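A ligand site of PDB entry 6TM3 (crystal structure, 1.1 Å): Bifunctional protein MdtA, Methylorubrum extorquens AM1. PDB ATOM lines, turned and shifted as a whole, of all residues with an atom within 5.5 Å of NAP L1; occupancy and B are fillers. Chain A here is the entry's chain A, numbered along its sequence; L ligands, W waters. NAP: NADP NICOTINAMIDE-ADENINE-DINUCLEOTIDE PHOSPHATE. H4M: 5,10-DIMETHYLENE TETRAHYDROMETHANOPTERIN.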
ATOM      1  N   GLY A  68     -23.798  -9.559 -18.026  1.00  0.00           N
ATOM      2  CA  GLY A  68     -23.825  -8.138 -17.716  1.00  0.00           C
ATOM      3  C   GLY A  68     -22.519  -7.534 -17.272  1.00  0.00           C
ATOM      4  O   GLY A  68     -22.468  -6.342 -16.967  1.00  0.00           O
ATOM      5  N   ASN A  97     -24.603  -8.344 -22.912  1.00  0.00           N
ATOM      6  CA  ASN A  97     -25.523  -7.227 -22.740  1.00  0.00           C
ATOM      7  C   ASN A  97     -25.700  -6.415 -24.021  1.00  0.00           C
ATOM      8  O   ASN A  97     -26.149  -5.276 -23.986  1.00  0.00           O
ATOM      9  CB  ASN A  97     -25.083  -6.326 -21.562  1.00  0.00           C
ATOM     10  CG  ASN A  97     -25.888  -6.528 -20.293  1.00  0.00           C
ATOM     11  OD1 ASN A  97     -26.575  -7.552 -20.099  1.00  0.00           O
ATOM     12  ND2 ASN A  97     -25.787  -5.561 -19.379  1.00  0.00           N
ATOM     13  N   GLY A  98     -25.378  -7.006 -25.163  1.00  0.00           N
ATOM     14  CA  GLY A  98     -25.401  -6.272 -26.417  1.00  0.00           C
ATOM     15  C   GLY A  98     -24.198  -5.397 -26.659  1.00  0.00           C
ATOM     16  O   GLY A  98     -24.210  -4.594 -27.581  1.00  0.00           O
ATOM     17  N   THR A 102     -24.226  -3.447 -30.135  1.00  0.00           N
ATOM     18  CA  THR A 102     -24.744  -2.092 -30.040  1.00  0.00           C
ATOM     19  C   THR A 102     -23.631  -1.057 -30.097  1.00  0.00           C
ATOM     20  O   THR A 102     -23.827  -0.021 -30.746  1.00  0.00           O
ATOM     21  CB  THR A 102     -25.670  -1.810 -28.859  1.00  0.00           C
ATOM     22  OG1 THR A 102     -26.545  -0.718 -29.203  1.00  0.00           O
ATOM     23  CG2 THR A 102     -24.888  -1.399 -27.610  1.00  0.00           C
ATOM     24  N   ALA A 127     -21.609   7.240 -18.114  1.00  0.00           N
ATOM     25  CA  ALA A 127     -21.990   5.946 -17.545  1.00  0.00           C
ATOM     26  C   ALA A 127     -21.383   4.804 -18.347  1.00  0.00           C
ATOM     27  O   ALA A 127     -22.038   3.812 -18.669  1.00  0.00           O
ATOM     28  CB  ALA A 127     -23.506   5.807 -17.431  1.00  0.00           C
ATOM     29  N   GLY A 128     -20.108   4.939 -18.652  1.00  0.00           N
ATOM     30  CA  GLY A 128     -19.424   4.067 -19.588  1.00  0.00           C
ATOM     31  C   GLY A 128     -18.872   2.787 -19.030  1.00  0.00           C
ATOM     32  O   GLY A 128     -18.111   2.101 -19.728  1.00  0.00           O
ATOM     33  N   THR A 129     -19.242   2.435 -17.803  1.00  0.00           N
ATOM     34  CA  THR A 129     -18.662   1.303 -17.089  1.00  0.00           C
ATOM     35  C   THR A 129     -19.401  -0.007 -17.303  1.00  0.00           C
ATOM     36  O   THR A 129     -18.907  -1.043 -16.850  1.00  0.00           O
ATOM     37  CB  THR A 129     -18.617   1.647 -15.604  1.00  0.00           C
ATOM     38  OG1 THR A 129     -19.945   2.042 -15.220  1.00  0.00           O
ATOM     39  CG2 THR A 129     -17.640   2.768 -15.297  1.00  0.00           C
ATOM     40  N   GLY A 130     -20.565  -0.012 -17.952  1.00  0.00           N
ATOM     41  CA  GLY A 130     -21.198  -1.250 -18.306  1.00  0.00           C
ATOM     42  C   GLY A 130     -20.642  -1.779 -19.607  1.00  0.00           C
ATOM     43  O   GLY A 130     -19.803  -1.156 -20.268  1.00  0.00           O
ATOM     44  N   PRO A 131     -21.128  -2.951 -20.019  1.00  0.00           N
ATOM     45  CA  PRO A 131     -20.609  -3.553 -21.256  1.00  0.00           C
ATOM     46  C   PRO A 131     -20.743  -2.656 -22.475  1.00  0.00           C
ATOM     47  O   PRO A 131     -19.831  -2.602 -23.308  1.00  0.00           O
ATOM     48  CB  PRO A 131     -21.405  -4.850 -21.378  1.00  0.00           C
ATOM     49  CG  PRO A 131     -21.750  -5.183 -19.939  1.00  0.00           C
ATOM     50  CD  PRO A 131     -22.026  -3.858 -19.284  1.00  0.00           C
ATOM     51  N   VAL A 132     -21.866  -1.951 -22.615  1.00  0.00           N
ATOM     52  CA  VAL A 132     -22.065  -1.135 -23.802  1.00  0.00           C
ATOM     53  C   VAL A 132     -21.133   0.065 -23.812  1.00  0.00           C
ATOM     54  O   VAL A 132     -20.554   0.404 -24.844  1.00  0.00           O
ATOM     55  CB  VAL A 132     -23.552  -0.701 -23.872  1.00  0.00           C
ATOM     56  CG1 VAL A 132     -23.763   0.343 -24.960  1.00  0.00           C
ATOM     57  CG2 VAL A 132     -24.435  -1.918 -24.071  1.00  0.00           C
ATOM     58  N   GLY A 133     -20.994   0.745 -22.672  1.00  0.00           N
ATOM     59  CA  GLY A 133     -20.075   1.867 -22.613  1.00  0.00           C
ATOM     60  C   GLY A 133     -18.630   1.447 -22.816  1.00  0.00           C
ATOM     61  O   GLY A 133     -17.858   2.148 -23.480  1.00  0.00           O
ATOM     62  N   CYS A 150     -16.644   7.721 -18.206  1.00  0.00           N
ATOM     63  CA  CYS A 150     -17.056   8.311 -16.944  1.00  0.00           C
ATOM     64  C   CYS A 150     -18.004   7.388 -16.181  1.00  0.00           C
ATOM     65  O   CYS A 150     -18.760   6.613 -16.769  1.00  0.00           O
ATOM     66  CB  CYS A 150     -17.805   9.637 -17.165  1.00  0.00           C
ATOM     67  SG  CYS A 150     -16.927  10.839 -18.140  1.00  0.00           S
ATOM     68  N   GLY A 151     -17.978   7.506 -14.854  1.00  0.00           N
ATOM     69  CA  GLY A 151     -18.962   6.865 -14.000  1.00  0.00           C
ATOM     70  C   GLY A 151     -19.048   7.608 -12.690  1.00  0.00           C
ATOM     71  O   GLY A 151     -18.277   8.540 -12.430  1.00  0.00           O
ATOM     72  N   ARG A 152     -19.988   7.187 -11.842  1.00  0.00           N
ATOM     73  CA  ARG A 152     -20.229   7.901 -10.602  1.00  0.00           C
ATOM     74  C   ARG A 152     -19.044   7.830  -9.642  1.00  0.00           C
ATOM     75  O   ARG A 152     -18.904   8.741  -8.807  1.00  0.00           O
ATOM     76  CB  ARG A 152     -21.485   7.371  -9.907  1.00  0.00           C
ATOM     77  CG  ARG A 152     -22.764   7.807 -10.601  1.00  0.00           C
ATOM     78  CD  ARG A 152     -23.981   7.053 -10.097  1.00  0.00           C
ATOM     79  NE  ARG A 152     -23.880   5.636 -10.440  1.00  0.00           N
ATOM     80  CZ  ARG A 152     -24.669   4.688  -9.981  1.00  0.00           C
ATOM     81  NH1 ARG A 152     -25.680   4.991  -9.190  1.00  0.00           N
ATOM     82  NH2 ARG A 152     -24.458   3.433 -10.344  1.00  0.00           N
ATOM     83  N   LYS A 153     -18.235   6.779  -9.711  1.00  0.00           N
ATOM     84  CA  LYS A 153     -17.116   6.571  -8.801  1.00  0.00           C
ATOM     85  C   LYS A 153     -15.857   6.331  -9.606  1.00  0.00           C
ATOM     86  O   LYS A 153     -15.830   5.475 -10.499  1.00  0.00           O
ATOM     87  CB  LYS A 153     -17.390   5.368  -7.882  1.00  0.00           C
ATOM     88  CG  LYS A 153     -18.536   5.610  -6.901  1.00  0.00           C
ATOM     89  CD  LYS A 153     -18.792   4.396  -6.018  1.00  0.00           C
ATOM     90  CE  LYS A 153     -19.773   4.748  -4.904  1.00  0.00           C
ATOM     91  NZ  LYS A 153     -20.295   3.533  -4.218  1.00  0.00           N
ATOM     92  N   LYS A 156     -14.310   2.556 -10.134  1.00  0.00           N
ATOM     93  CA  LYS A 156     -15.030   1.705 -11.082  1.00  0.00           C
ATOM     94  C   LYS A 156     -14.811   2.175 -12.518  1.00  0.00           C
ATOM     95  O   LYS A 156     -14.655   1.354 -13.421  1.00  0.00           O
ATOM     96  CB  LYS A 156     -16.511   1.666 -10.694  1.00  0.00           C
ATOM     97  CG  LYS A 156     -17.375   0.818 -11.608  1.00  0.00           C
ATOM     98  CD  LYS A 156     -18.827   0.797 -11.115  1.00  0.00           C
ATOM     99  CE  LYS A 156     -19.762   0.054 -12.036  1.00  0.00           C
ATOM    100  NZ  LYS A 156     -21.166   0.129 -11.516  1.00  0.00           N
ATOM    101  N   ALA A 157     -14.774   3.492 -12.742  1.00  0.00           N
ATOM    102  CA  ALA A 157     -14.473   4.022 -14.076  1.00  0.00           C
ATOM    103  C   ALA A 157     -13.062   3.647 -14.488  1.00  0.00           C
ATOM    104  O   ALA A 157     -12.829   3.273 -15.644  1.00  0.00           O
ATOM    105  CB  ALA A 157     -14.698   5.532 -14.092  1.00  0.00           C
ATOM    106  N   ARG A 183     -21.461  15.603 -14.760  1.00  0.00           N
ATOM    107  CA  ARG A 183     -21.618  15.098 -16.118  1.00  0.00           C
ATOM    108  C   ARG A 183     -21.660  16.253 -17.119  1.00  0.00           C
ATOM    109  O   ARG A 183     -21.082  16.182 -18.200  1.00  0.00           O
ATOM    110  CB  ARG A 183     -22.869  14.226 -16.216  1.00  0.00           C
ATOM    111  CG  ARG A 183     -22.737  12.878 -15.543  1.00  0.00           C
ATOM    112  CD  ARG A 183     -23.852  11.931 -15.931  1.00  0.00           C
ATOM    113  NE  ARG A 183     -25.135  12.334 -15.371  1.00  0.00           N
ATOM    114  CZ  ARG A 183     -25.590  11.952 -14.189  1.00  0.00           C
ATOM    115  NH1 ARG A 183     -24.881  11.123 -13.415  1.00  0.00           N
ATOM    116  NH2 ARG A 183     -26.775  12.374 -13.781  1.00  0.00           N
ATOM    117  N   ALA A 196     -24.423   5.806 -22.077  1.00  0.00           N
ATOM    118  CA  ALA A 196     -24.534   4.354 -21.933  1.00  0.00           C
ATOM    119  C   ALA A 196     -25.025   3.977 -20.533  1.00  0.00           C
ATOM    120  O   ALA A 196     -24.624   2.954 -19.961  1.00  0.00           O
ATOM    121  CB  ALA A 196     -23.203   3.680 -22.260  1.00  0.00           C
ATOM    122  N   GLY A 197     -25.921   4.798 -19.985  1.00  0.00           N
ATOM    123  CA  GLY A 197     -26.445   4.542 -18.664  1.00  0.00           C
ATOM    124  C   GLY A 197     -27.430   3.394 -18.645  1.00  0.00           C
ATOM    125  O   GLY A 197     -28.011   3.005 -19.646  1.00  0.00           O
ATOM    126  N   ALA A 198     -27.630   2.873 -17.436  1.00  0.00           N
ATOM    127  CA  ALA A 198     -28.618   1.843 -17.194  1.00  0.00           C
ATOM    128  C   ALA A 198     -30.009   2.293 -17.639  1.00  0.00           C
ATOM    129  O   ALA A 198     -30.322   3.479 -17.793  1.00  0.00           O
ATOM    130  CB  ALA A 198     -28.631   1.467 -15.718  1.00  0.00           C
ATOM    131  N   ILE A 199     -30.866   1.309 -17.845  1.00  0.00           N
ATOM    132  CA  ILE A 199     -32.132   1.524 -18.529  1.00  0.00           C
ATOM    133  C   ILE A 199     -33.026   2.479 -17.745  1.00  0.00           C
ATOM    134  O   ILE A 199     -33.112   2.442 -16.511  1.00  0.00           O
ATOM    135  CB  ILE A 199     -32.801   0.160 -18.778  1.00  0.00           C
ATOM    136  CG1 ILE A 199     -34.055   0.296 -19.632  1.00  0.00           C
ATOM    137  CG2 ILE A 199     -33.112  -0.598 -17.473  1.00  0.00           C
ATOM    138  CD1 ILE A 199     -34.489  -1.018 -20.281  1.00  0.00           C
ATOM    139  N   GLY A 200     -33.678   3.370 -18.482  1.00  0.00           N
ATOM    140  CA  GLY A 200     -34.670   4.231 -17.882  1.00  0.00           C
ATOM    141  C   GLY A 200     -34.139   5.392 -17.072  1.00  0.00           C
ATOM    142  O   GLY A 200     -34.855   5.872 -16.184  1.00  0.00           O
ATOM    143  N   LEU A 201     -32.938   5.863 -17.376  1.00  0.00           N
ATOM    144  CA  LEU A 201     -32.317   6.970 -16.670  1.00  0.00           C
ATOM    145  C   LEU A 201     -31.887   8.062 -17.643  1.00  0.00           C
ATOM    146  O   LEU A 201     -31.300   7.775 -18.682  1.00  0.00           O
ATOM    147  CB  LEU A 201     -31.033   6.493 -15.969  1.00  0.00           C
ATOM    148  CG  LEU A 201     -31.215   5.431 -14.886  1.00  0.00           C
ATOM    149  CD1 LEU A 201     -29.855   4.957 -14.426  1.00  0.00           C
ATOM    150  CD2 LEU A 201     -32.015   5.984 -13.719  1.00  0.00           C
ATOM    151  N   LEU A 203     -29.186  10.872 -18.302  1.00  0.00           N
ATOM    152  CA  LEU A 203     -27.844  11.250 -17.905  1.00  0.00           C
ATOM    153  C   LEU A 203     -27.423  12.629 -18.366  1.00  0.00           C
ATOM    154  O   LEU A 203     -26.544  13.243 -17.744  1.00  0.00           O
ATOM    155  CB  LEU A 203     -26.821  10.275 -18.477  1.00  0.00           C
ATOM    156  CG  LEU A 203     -26.847   8.885 -17.863  1.00  0.00           C
ATOM    157  CD1 LEU A 203     -25.818   8.084 -18.588  1.00  0.00           C
ATOM    158  CD2 LEU A 203     -26.565   8.927 -16.378  1.00  0.00           C
ATOM    159  N   ASP A 220     -27.364   8.112 -27.804  1.00  0.00           N
ATOM    160  CA  ASP A 220     -27.940   7.578 -26.575  1.00  0.00           C
ATOM    161  C   ASP A 220     -28.386   6.143 -26.798  1.00  0.00           C
ATOM    162  O   ASP A 220     -29.124   5.865 -27.745  1.00  0.00           O
ATOM    163  CB  ASP A 220     -29.146   8.443 -26.172  1.00  0.00           C
ATOM    164  CG  ASP A 220     -29.859   7.947 -24.919  1.00  0.00           C
ATOM    165  OD1 ASP A 220     -29.275   7.203 -24.103  1.00  0.00           O
ATOM    166  OD2 ASP A 220     -31.041   8.352 -24.739  1.00  0.00           O
ATOM    167  N   TYR A 221     -27.945   5.246 -25.927  1.00  0.00           N
ATOM    168  CA  TYR A 221     -28.330   3.856 -26.037  1.00  0.00           C
ATOM    169  C   TYR A 221     -29.604   3.498 -25.279  1.00  0.00           C
ATOM    170  O   TYR A 221     -30.169   2.439 -25.534  1.00  0.00           O
ATOM    171  CB  TYR A 221     -27.196   2.971 -25.550  1.00  0.00           C
ATOM    172  CG  TYR A 221     -25.947   3.025 -26.405  1.00  0.00           C
ATOM    173  CD1 TYR A 221     -25.918   2.434 -27.666  1.00  0.00           C
ATOM    174  CD2 TYR A 221     -24.792   3.628 -25.944  1.00  0.00           C
ATOM    175  CE1 TYR A 221     -24.784   2.437 -28.426  1.00  0.00           C
ATOM    176  CE2 TYR A 221     -23.640   3.634 -26.705  1.00  0.00           C
ATOM    177  CZ  TYR A 221     -23.633   3.035 -27.944  1.00  0.00           C
ATOM    178  OH  TYR A 221     -22.502   3.013 -28.730  1.00  0.00           O
ATOM    179  N   ASN A 222     -30.068   4.323 -24.346  1.00  0.00           N
ATOM    180  CA  ASN A 222     -31.198   3.935 -23.510  1.00  0.00           C
ATOM    181  C   ASN A 222     -32.516   4.143 -24.255  1.00  0.00           C
ATOM    182  O   ASN A 222     -32.867   5.275 -24.603  1.00  0.00           O
ATOM    183  CB  ASN A 222     -31.209   4.781 -22.241  1.00  0.00           C
ATOM    184  CG  ASN A 222     -32.466   4.591 -21.432  1.00  0.00           C
ATOM    185  OD1 ASN A 222     -32.964   3.473 -21.296  1.00  0.00           O
ATOM    186  ND2 ASN A 222     -32.986   5.682 -20.908  1.00  0.00           N
ATOM    187  N   ALA A 223     -33.268   3.060 -24.432  1.00  0.00           N
ATOM    188  CA  ALA A 223     -34.554   3.098 -25.132  1.00  0.00           C
ATOM    189  C   ALA A 223     -35.750   3.310 -24.220  1.00  0.00           C
ATOM    190  O   ALA A 223     -36.832   3.631 -24.722  1.00  0.00           O
ATOM    191  CB  ALA A 223     -34.760   1.801 -25.903  1.00  0.00           C
ATOM    192  N   ALA A 249     -31.809   5.752 -29.175  1.00  0.00           N
ATOM    193  CA  ALA A 249     -31.602   4.339 -28.922  1.00  0.00           C
ATOM    194  C   ALA A 249     -32.267   3.452 -29.964  1.00  0.00           C
ATOM    195  O   ALA A 249     -31.787   2.356 -30.236  1.00  0.00           O
ATOM    196  CB  ALA A 249     -32.150   3.994 -27.551  1.00  0.00           C
ATOM    197  N   LEU A 250     -33.419   3.875 -30.497  1.00  0.00           N
ATOM    198  CA  LEU A 250     -34.076   3.078 -31.527  1.00  0.00           C
ATOM    199  C   LEU A 250     -33.429   3.263 -32.892  1.00  0.00           C
ATOM    200  O   LEU A 250     -33.408   2.318 -33.698  1.00  0.00           O
ATOM    201  CB  LEU A 250     -35.572   3.388 -31.608  1.00  0.00           C
ATOM    202  CG  LEU A 250     -36.362   3.110 -30.324  1.00  0.00           C
ATOM    203  CD1 LEU A 250     -37.846   3.443 -30.558  1.00  0.00           C
ATOM    204  CD2 LEU A 250     -36.226   1.708 -29.779  1.00  0.00           C
ATOM    205  N   ILE A 252     -30.190   3.639 -33.262  1.00  0.00           N
ATOM    206  CA  ILE A 252     -29.054   2.725 -33.138  1.00  0.00           C
ATOM    207  C   ILE A 252     -29.536   1.293 -33.106  1.00  0.00           C
ATOM    208  O   ILE A 252     -28.949   0.410 -33.742  1.00  0.00           O
ATOM    209  CB  ILE A 252     -28.271   3.076 -31.860  1.00  0.00           C
ATOM    210  CG1 ILE A 252     -27.635   4.462 -31.990  1.00  0.00           C
ATOM    211  CG2 ILE A 252     -27.209   2.021 -31.559  1.00  0.00           C
ATOM    212  CD1 ILE A 252     -27.136   5.013 -30.689  1.00  0.00           C
ATOM    213  N   GLY A 253     -30.619   1.043 -32.356  1.00  0.00           N
ATOM    214  CA  GLY A 253     -31.070  -0.313 -32.112  1.00  0.00           C
ATOM    215  C   GLY A 253     -31.487  -1.069 -33.355  1.00  0.00           C
ATOM    216  O   GLY A 253     -31.344  -2.283 -33.415  1.00  0.00           O
ATOM    217  N   LYS A 256     -28.318  -2.339 -34.638  1.00  0.00           N
ATOM    218  CA  LYS A 256     -27.809  -3.367 -33.687  1.00  0.00           C
ATOM    219  C   LYS A 256     -28.544  -4.705 -33.898  1.00  0.00           C
ATOM    220  O   LYS A 256     -27.920  -5.749 -33.914  1.00  0.00           O
ATOM    221  CB  LYS A 256     -27.939  -2.877 -32.247  1.00  0.00           C
ATOM    222  CG  LYS A 256     -27.677  -3.963 -31.195  1.00  0.00           C
ATOM    223  CD  LYS A 256     -28.969  -4.620 -30.700  1.00  0.00           C
ATOM    224  CE  LYS A 256     -28.923  -6.137 -30.637  1.00  0.00           C
ATOM    225  NZ  LYS A 256     -27.957  -6.674 -29.642  1.00  0.00           N
HETATM  226  PA  NAP L   1     -25.678  -1.304 -17.426  1.00  0.00           P
HETATM  227  O1A NAP L   1     -24.468  -2.151 -17.242  1.00  0.00           O
HETATM  228  O2A NAP L   1     -26.971  -1.852 -16.926  1.00  0.00           O
HETATM  229  O5B NAP L   1     -25.490   0.127 -16.760  1.00  0.00           O
HETATM  230  C5B NAP L   1     -24.476   0.988 -17.254  1.00  0.00           C
HETATM  231  C4B NAP L   1     -23.991   1.928 -16.194  1.00  0.00           C
HETATM  232  O4B NAP L   1     -25.042   2.814 -15.770  1.00  0.00           O
HETATM  233  C3B NAP L   1     -23.522   1.314 -14.868  1.00  0.00           C
HETATM  234  O3B NAP L   1     -22.279   0.643 -14.952  1.00  0.00           O
HETATM  235  C2B NAP L   1     -23.530   2.529 -13.948  1.00  0.00           C
HETATM  236  O2B NAP L   1     -22.255   3.159 -14.002  1.00  0.00           O
HETATM  237  C1B NAP L   1     -24.579   3.452 -14.585  1.00  0.00           C
HETATM  238  N9A NAP L   1     -25.712   3.719 -13.693  1.00  0.00           N
HETATM  239  C8A NAP L   1     -26.481   2.780 -13.086  1.00  0.00           C
HETATM  240  N7A NAP L   1     -27.394   3.389 -12.294  1.00  0.00           N
HETATM  241  C5A NAP L   1     -27.175   4.710 -12.392  1.00  0.00           C
HETATM  242  C6A NAP L   1     -27.764   5.909 -11.812  1.00  0.00           C
HETATM  243  N6A NAP L   1     -28.801   5.787 -10.953  1.00  0.00           N
HETATM  244  N1A NAP L   1     -27.243   7.091 -12.168  1.00  0.00           N
HETATM  245  C2A NAP L   1     -26.217   7.205 -13.022  1.00  0.00           C
HETATM  246  N3A NAP L   1     -25.626   6.151 -13.597  1.00  0.00           N
HETATM  247  C4A NAP L   1     -26.079   4.925 -13.302  1.00  0.00           C
HETATM  248  O3  NAP L   1     -25.835  -0.923 -18.972  1.00  0.00           O
HETATM  249  PN  NAP L   1     -25.191  -1.526 -20.317  1.00  0.00           P
HETATM  250  O1N NAP L   1     -25.410  -2.988 -20.405  1.00  0.00           O
HETATM  251  O2N NAP L   1     -23.803  -1.023 -20.444  1.00  0.00           O
HETATM  252  O5D NAP L   1     -26.151  -0.838 -21.366  1.00  0.00           O
HETATM  253  C5D NAP L   1     -26.205   0.591 -21.441  1.00  0.00           C
HETATM  254  C4D NAP L   1     -27.576   1.000 -21.941  1.00  0.00           C
HETATM  255  O4D NAP L   1     -27.734   0.559 -23.305  1.00  0.00           O
HETATM  256  C3D NAP L   1     -28.761   0.424 -21.169  1.00  0.00           C
HETATM  257  O3D NAP L   1     -29.798   1.393 -21.033  1.00  0.00           O
HETATM  258  C2D NAP L   1     -29.262  -0.702 -22.059  1.00  0.00           C
HETATM  259  O2D NAP L   1     -30.623  -1.023 -21.936  1.00  0.00           O
HETATM  260  C1D NAP L   1     -29.034  -0.092 -23.424  1.00  0.00           C
HETATM  261  N1N NAP L   1     -28.889  -0.922 -24.590  1.00  0.00           N
HETATM  262  C2N NAP L   1     -29.291  -0.416 -25.765  1.00  0.00           C
HETATM  263  C3N NAP L   1     -29.102  -1.121 -26.944  1.00  0.00           C
HETATM  264  C7N NAP L   1     -29.561  -0.547 -28.248  1.00  0.00           C
HETATM  265  O7N NAP L   1     -29.338  -1.164 -29.287  1.00  0.00           O
HETATM  266  N7N NAP L   1     -30.165   0.629 -28.226  1.00  0.00           N
HETATM  267  C4N NAP L   1     -28.429  -2.324 -26.904  1.00  0.00           C
HETATM  268  C5N NAP L   1     -27.979  -2.843 -25.707  1.00  0.00           C
HETATM  269  C6N NAP L   1     -28.160  -2.151 -24.473  1.00  0.00           C
HETATM  270  P2B NAP L   1     -21.486   3.701 -12.685  1.00  0.00           P
HETATM  271  O1X NAP L   1     -21.871   2.806 -11.521  1.00  0.00           O
HETATM  272  O2X NAP L   1     -20.029   3.594 -13.069  1.00  0.00           O
HETATM  273  O3X NAP L   1     -21.894   5.132 -12.445  1.00  0.00           O
HETATM  274  N1  H4M L   2     -29.852  -7.239 -23.624  1.00  0.00           N
HETATM  275  C2  H4M L   2     -28.945  -7.801 -24.435  1.00  0.00           C
HETATM  276  NA2 H4M L   2     -28.309  -8.932 -24.059  1.00  0.00           N
HETATM  277  N3  H4M L   2     -28.625  -7.266 -25.646  1.00  0.00           N
HETATM  278  C4  H4M L   2     -29.195  -6.119 -26.111  1.00  0.00           C
HETATM  279  OH4 H4M L   2     -28.821  -5.678 -27.219  1.00  0.00           O
HETATM  280  C4A H4M L   2     -30.178  -5.506 -25.282  1.00  0.00           C
HETATM  281  N5  H4M L   2     -30.836  -4.328 -25.615  1.00  0.00           N
HETATM  282  C6  H4M L   2     -31.617  -3.617 -24.615  1.00  0.00           C
HETATM  283  C7  H4M L   2     -32.344  -4.616 -23.707  1.00  0.00           C
HETATM  284  C7M H4M L   2     -32.984  -3.929 -22.535  1.00  0.00           C
HETATM  285  N8  H4M L   2     -31.395  -5.608 -23.220  1.00  0.00           N
HETATM  286  C8A H4M L   2     -30.471  -6.119 -24.035  1.00  0.00           C
HETATM  287  C9  H4M L   2     -32.559  -2.742 -25.431  1.00  0.00           C
HETATM  288  C9M H4M L   2     -32.628  -1.316 -24.895  1.00  0.00           C
HETATM  289  C10 H4M L   2     -31.099  -3.900 -26.944  1.00  0.00           C
HETATM  290  N10 H4M L   2     -32.048  -2.840 -26.801  1.00  0.00           N
HETATM  291  C11 H4M L   2     -34.240  -1.884 -30.233  1.00  0.00           C
HETATM  292  C12 H4M L   2     -34.731  -1.530 -28.998  1.00  0.00           C
HETATM  293  C13 H4M L   2     -34.015  -1.829 -27.838  1.00  0.00           C
HETATM  294  C14 H4M L   2     -32.815  -2.485 -27.928  1.00  0.00           C
HETATM  295  C15 H4M L   2     -32.336  -2.845 -29.195  1.00  0.00           C
HETATM  296  C16 H4M L   2     -33.039  -2.540 -30.323  1.00  0.00           C
HETATM  297  CX1 H4M L   2     -35.019  -1.552 -31.513  1.00  0.00           C
HETATM  298  CX2 H4M L   2     -36.295  -2.334 -31.717  1.00  0.00           C
HETATM  299  CX3 H4M L   2     -36.983  -1.846 -33.041  1.00  0.00           C
HETATM  300  CX4 H4M L   2     -38.151  -2.692 -33.484  1.00  0.00           C
HETATM  301  CX5 H4M L   2     -37.528  -3.901 -34.161  1.00  0.00           C
HETATM  302  OX2 H4M L   2     -35.951  -3.725 -31.724  1.00  0.00           O
HETATM  303  OX3 H4M L   2     -37.376  -0.494 -32.810  1.00  0.00           O
HETATM  304  OX5 H4M L   2     -37.597  -5.047 -33.409  1.00  0.00           O
HETATM  305  O   HOH W   1     -22.929   6.842 -14.241  1.00  0.00           O
HETATM  306  O   HOH W   2     -27.484  -3.940 -21.922  1.00  0.00           O
HETATM  307  O   HOH W   3     -27.296  -2.121 -14.235  1.00  0.00           O
HETATM  308  O   HOH W   4     -22.247   1.160 -20.019  1.00  0.00           O
HETATM  309  O   HOH W   5     -29.777   1.708 -12.250  1.00  0.00           O
HETATM  310  O   HOH W   6     -18.492   4.398 -11.088  1.00  0.00           O
HETATM  311  O   HOH W   7     -32.505   0.986 -22.595  1.00  0.00           O
HETATM  312  O   HOH W   8     -24.612  -4.741 -16.322  1.00  0.00           O
HETATM  313  O   HOH W   9     -27.920  -4.499 -17.523  1.00  0.00           O
HETATM  314  O   HOH W  10     -30.827  -2.653 -19.713  1.00  0.00           O
HETATM  315  O   HOH W  11     -29.632  -1.364 -17.584  1.00  0.00           O
HETATM  316  O   HOH W  12     -27.857   9.102 -10.302  1.00  0.00           O
HETATM  317  O   HOH W  13     -30.417   8.147  -9.803  1.00  0.00           O
HETATM  318  O   HOH W  14     -22.597  -2.038 -15.293  1.00  0.00           O
HETATM  319  O   HOH W  15     -30.144   3.030  -9.867  1.00  0.00           O
HETATM  320  O   HOH W  16     -20.661   3.577  -9.204  1.00  0.00           O
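An oxygen (O2N) of NAP L1 lies close to the backbone nitrogen of Pro 131. Merely in contact with NAP L1: Ala 127 (3.7 Å), Gly 130 (3.4 Å), Gly 133 (3.998 Å), Gly 151 (3.6 Å), Ala 196 (3.2 Å), Leu 201 (3.4 Å), Leu 203 (3.8 Å), Asn 222 (3.8 Å), Gly 253 (3.4 Å) and Lys 256 (3.7 Å). The nearest printed residue that does not touch NAP L1 is Arg 183 (4.2 Å).
Water W6 lies within hydrogen-bond range of an oxygen (O2X) of NAP L1, the backbone NH (N) of Lys 153 and the backbone NH (N) of Arg 152. Water W4 lies within hydrogen-bond range of an oxygen (O2N) of NAP L1, the backbone NH (N) of Gly 130, the backbone NH (N) of Gly 133, the backbone carbonyl oxygen (O) of Ala 196 and the backbone carbonyl oxygen (O) of Ala 127. Water W2 lies within hydrogen-bond range of an oxygen (O1N) of NAP L1 (2.7 Å) and the backbone carbonyl oxygen of Asn 97 (2.8 Å). Water W8 lies within hydrogen-bond range of an oxygen (O1A) of NAP L1, the backbone carbonyl oxygen of Gly 68 and the side-chain amide nitrogen of Asn 97. Water W7 lies within hydrogen-bond range of O2D of NAP L1, OD1 of Asn 222 and N of Ala 223. Water W9 bridges an oxygen (O2A) of NAP L1 (2.9 Å) and the side-chain amide nitrogen (ND2) of Asn 97 (3.0 Å).
The backbone NH (N) of Ala 249 is in hydrogen-bond range of the backbone carbonyl oxygen (O) of Asp 220 (3.0 Å). The side-chain amide nitrogen of Asn 222 is in hydrogen-bond range of the backbone carbonyl oxygen of Leu 201 (3.5 Å). The backbone NH (N) of Ala 127 lies within hydrogen-bond range of the backbone carbonyl oxygen (O) of Cys 150. The backbone carbonyl oxygen of Leu 203 is in hydrogen-bond range of the guanidinium group of Arg 183, at 2.9 Å. The side-chain amide oxygen of Asn 222 lies within hydrogen-bond range of the backbone NH of Gly 200, 2.9 Å away. The side-chain carboxylate of Asp 220 is in hydrogen-bond range of the backbone NH of Asn 222 (3.0 Å).
OG1 of Thr 129 sits at hydrogen-bond distance from O2X of NAP L1 (2.7 Å). NZ of Lys 156 is in salt-bridge range of O1X of NAP L1. An oxygen (O3D) of NAP L1 is in hydrogen-bond range of the backbone carbonyl oxygen (O) of Gly 197 (2.8 Å). An oxygen (O1N) of NAP L1 is in hydrogen-bond range of the side-chain amide nitrogen (ND2) of Asn 97 (2.8 Å). The side-chain hydroxyl of Thr 102 is in hydrogen-bond range of an oxygen (O7N) of NAP L1, 2.8 Å away. O3X of NAP L1 sits at hydrogen-bond distance from N of Arg 152 (2.9 Å). NE of Arg 152 is in salt-bridge range of O3X of NAP L1, 2.9 Å away. O of Tyr 221 lies close to N7N of NAP L1, 3.2 Å away. O2N of NAP L1 is in hydrogen-bond range of N of Val 132, at 3.1 Å. The backbone NH (N) of Ala 198 sits at hydrogen-bond distance from an oxygen (O4B) of NAP L1 (3.1 Å). O of Ala 249 lies within hydrogen-bond range of N7N of NAP L1 (3.1 Å). N of Ile 199 lies within hydrogen-bond range of O3D of NAP L1 (3.4 Å). The side-chain amino group (NZ) of Lys 256 lies within hydrogen-bond range of an oxygen (OH4) of H4M L2 (2.8 Å).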
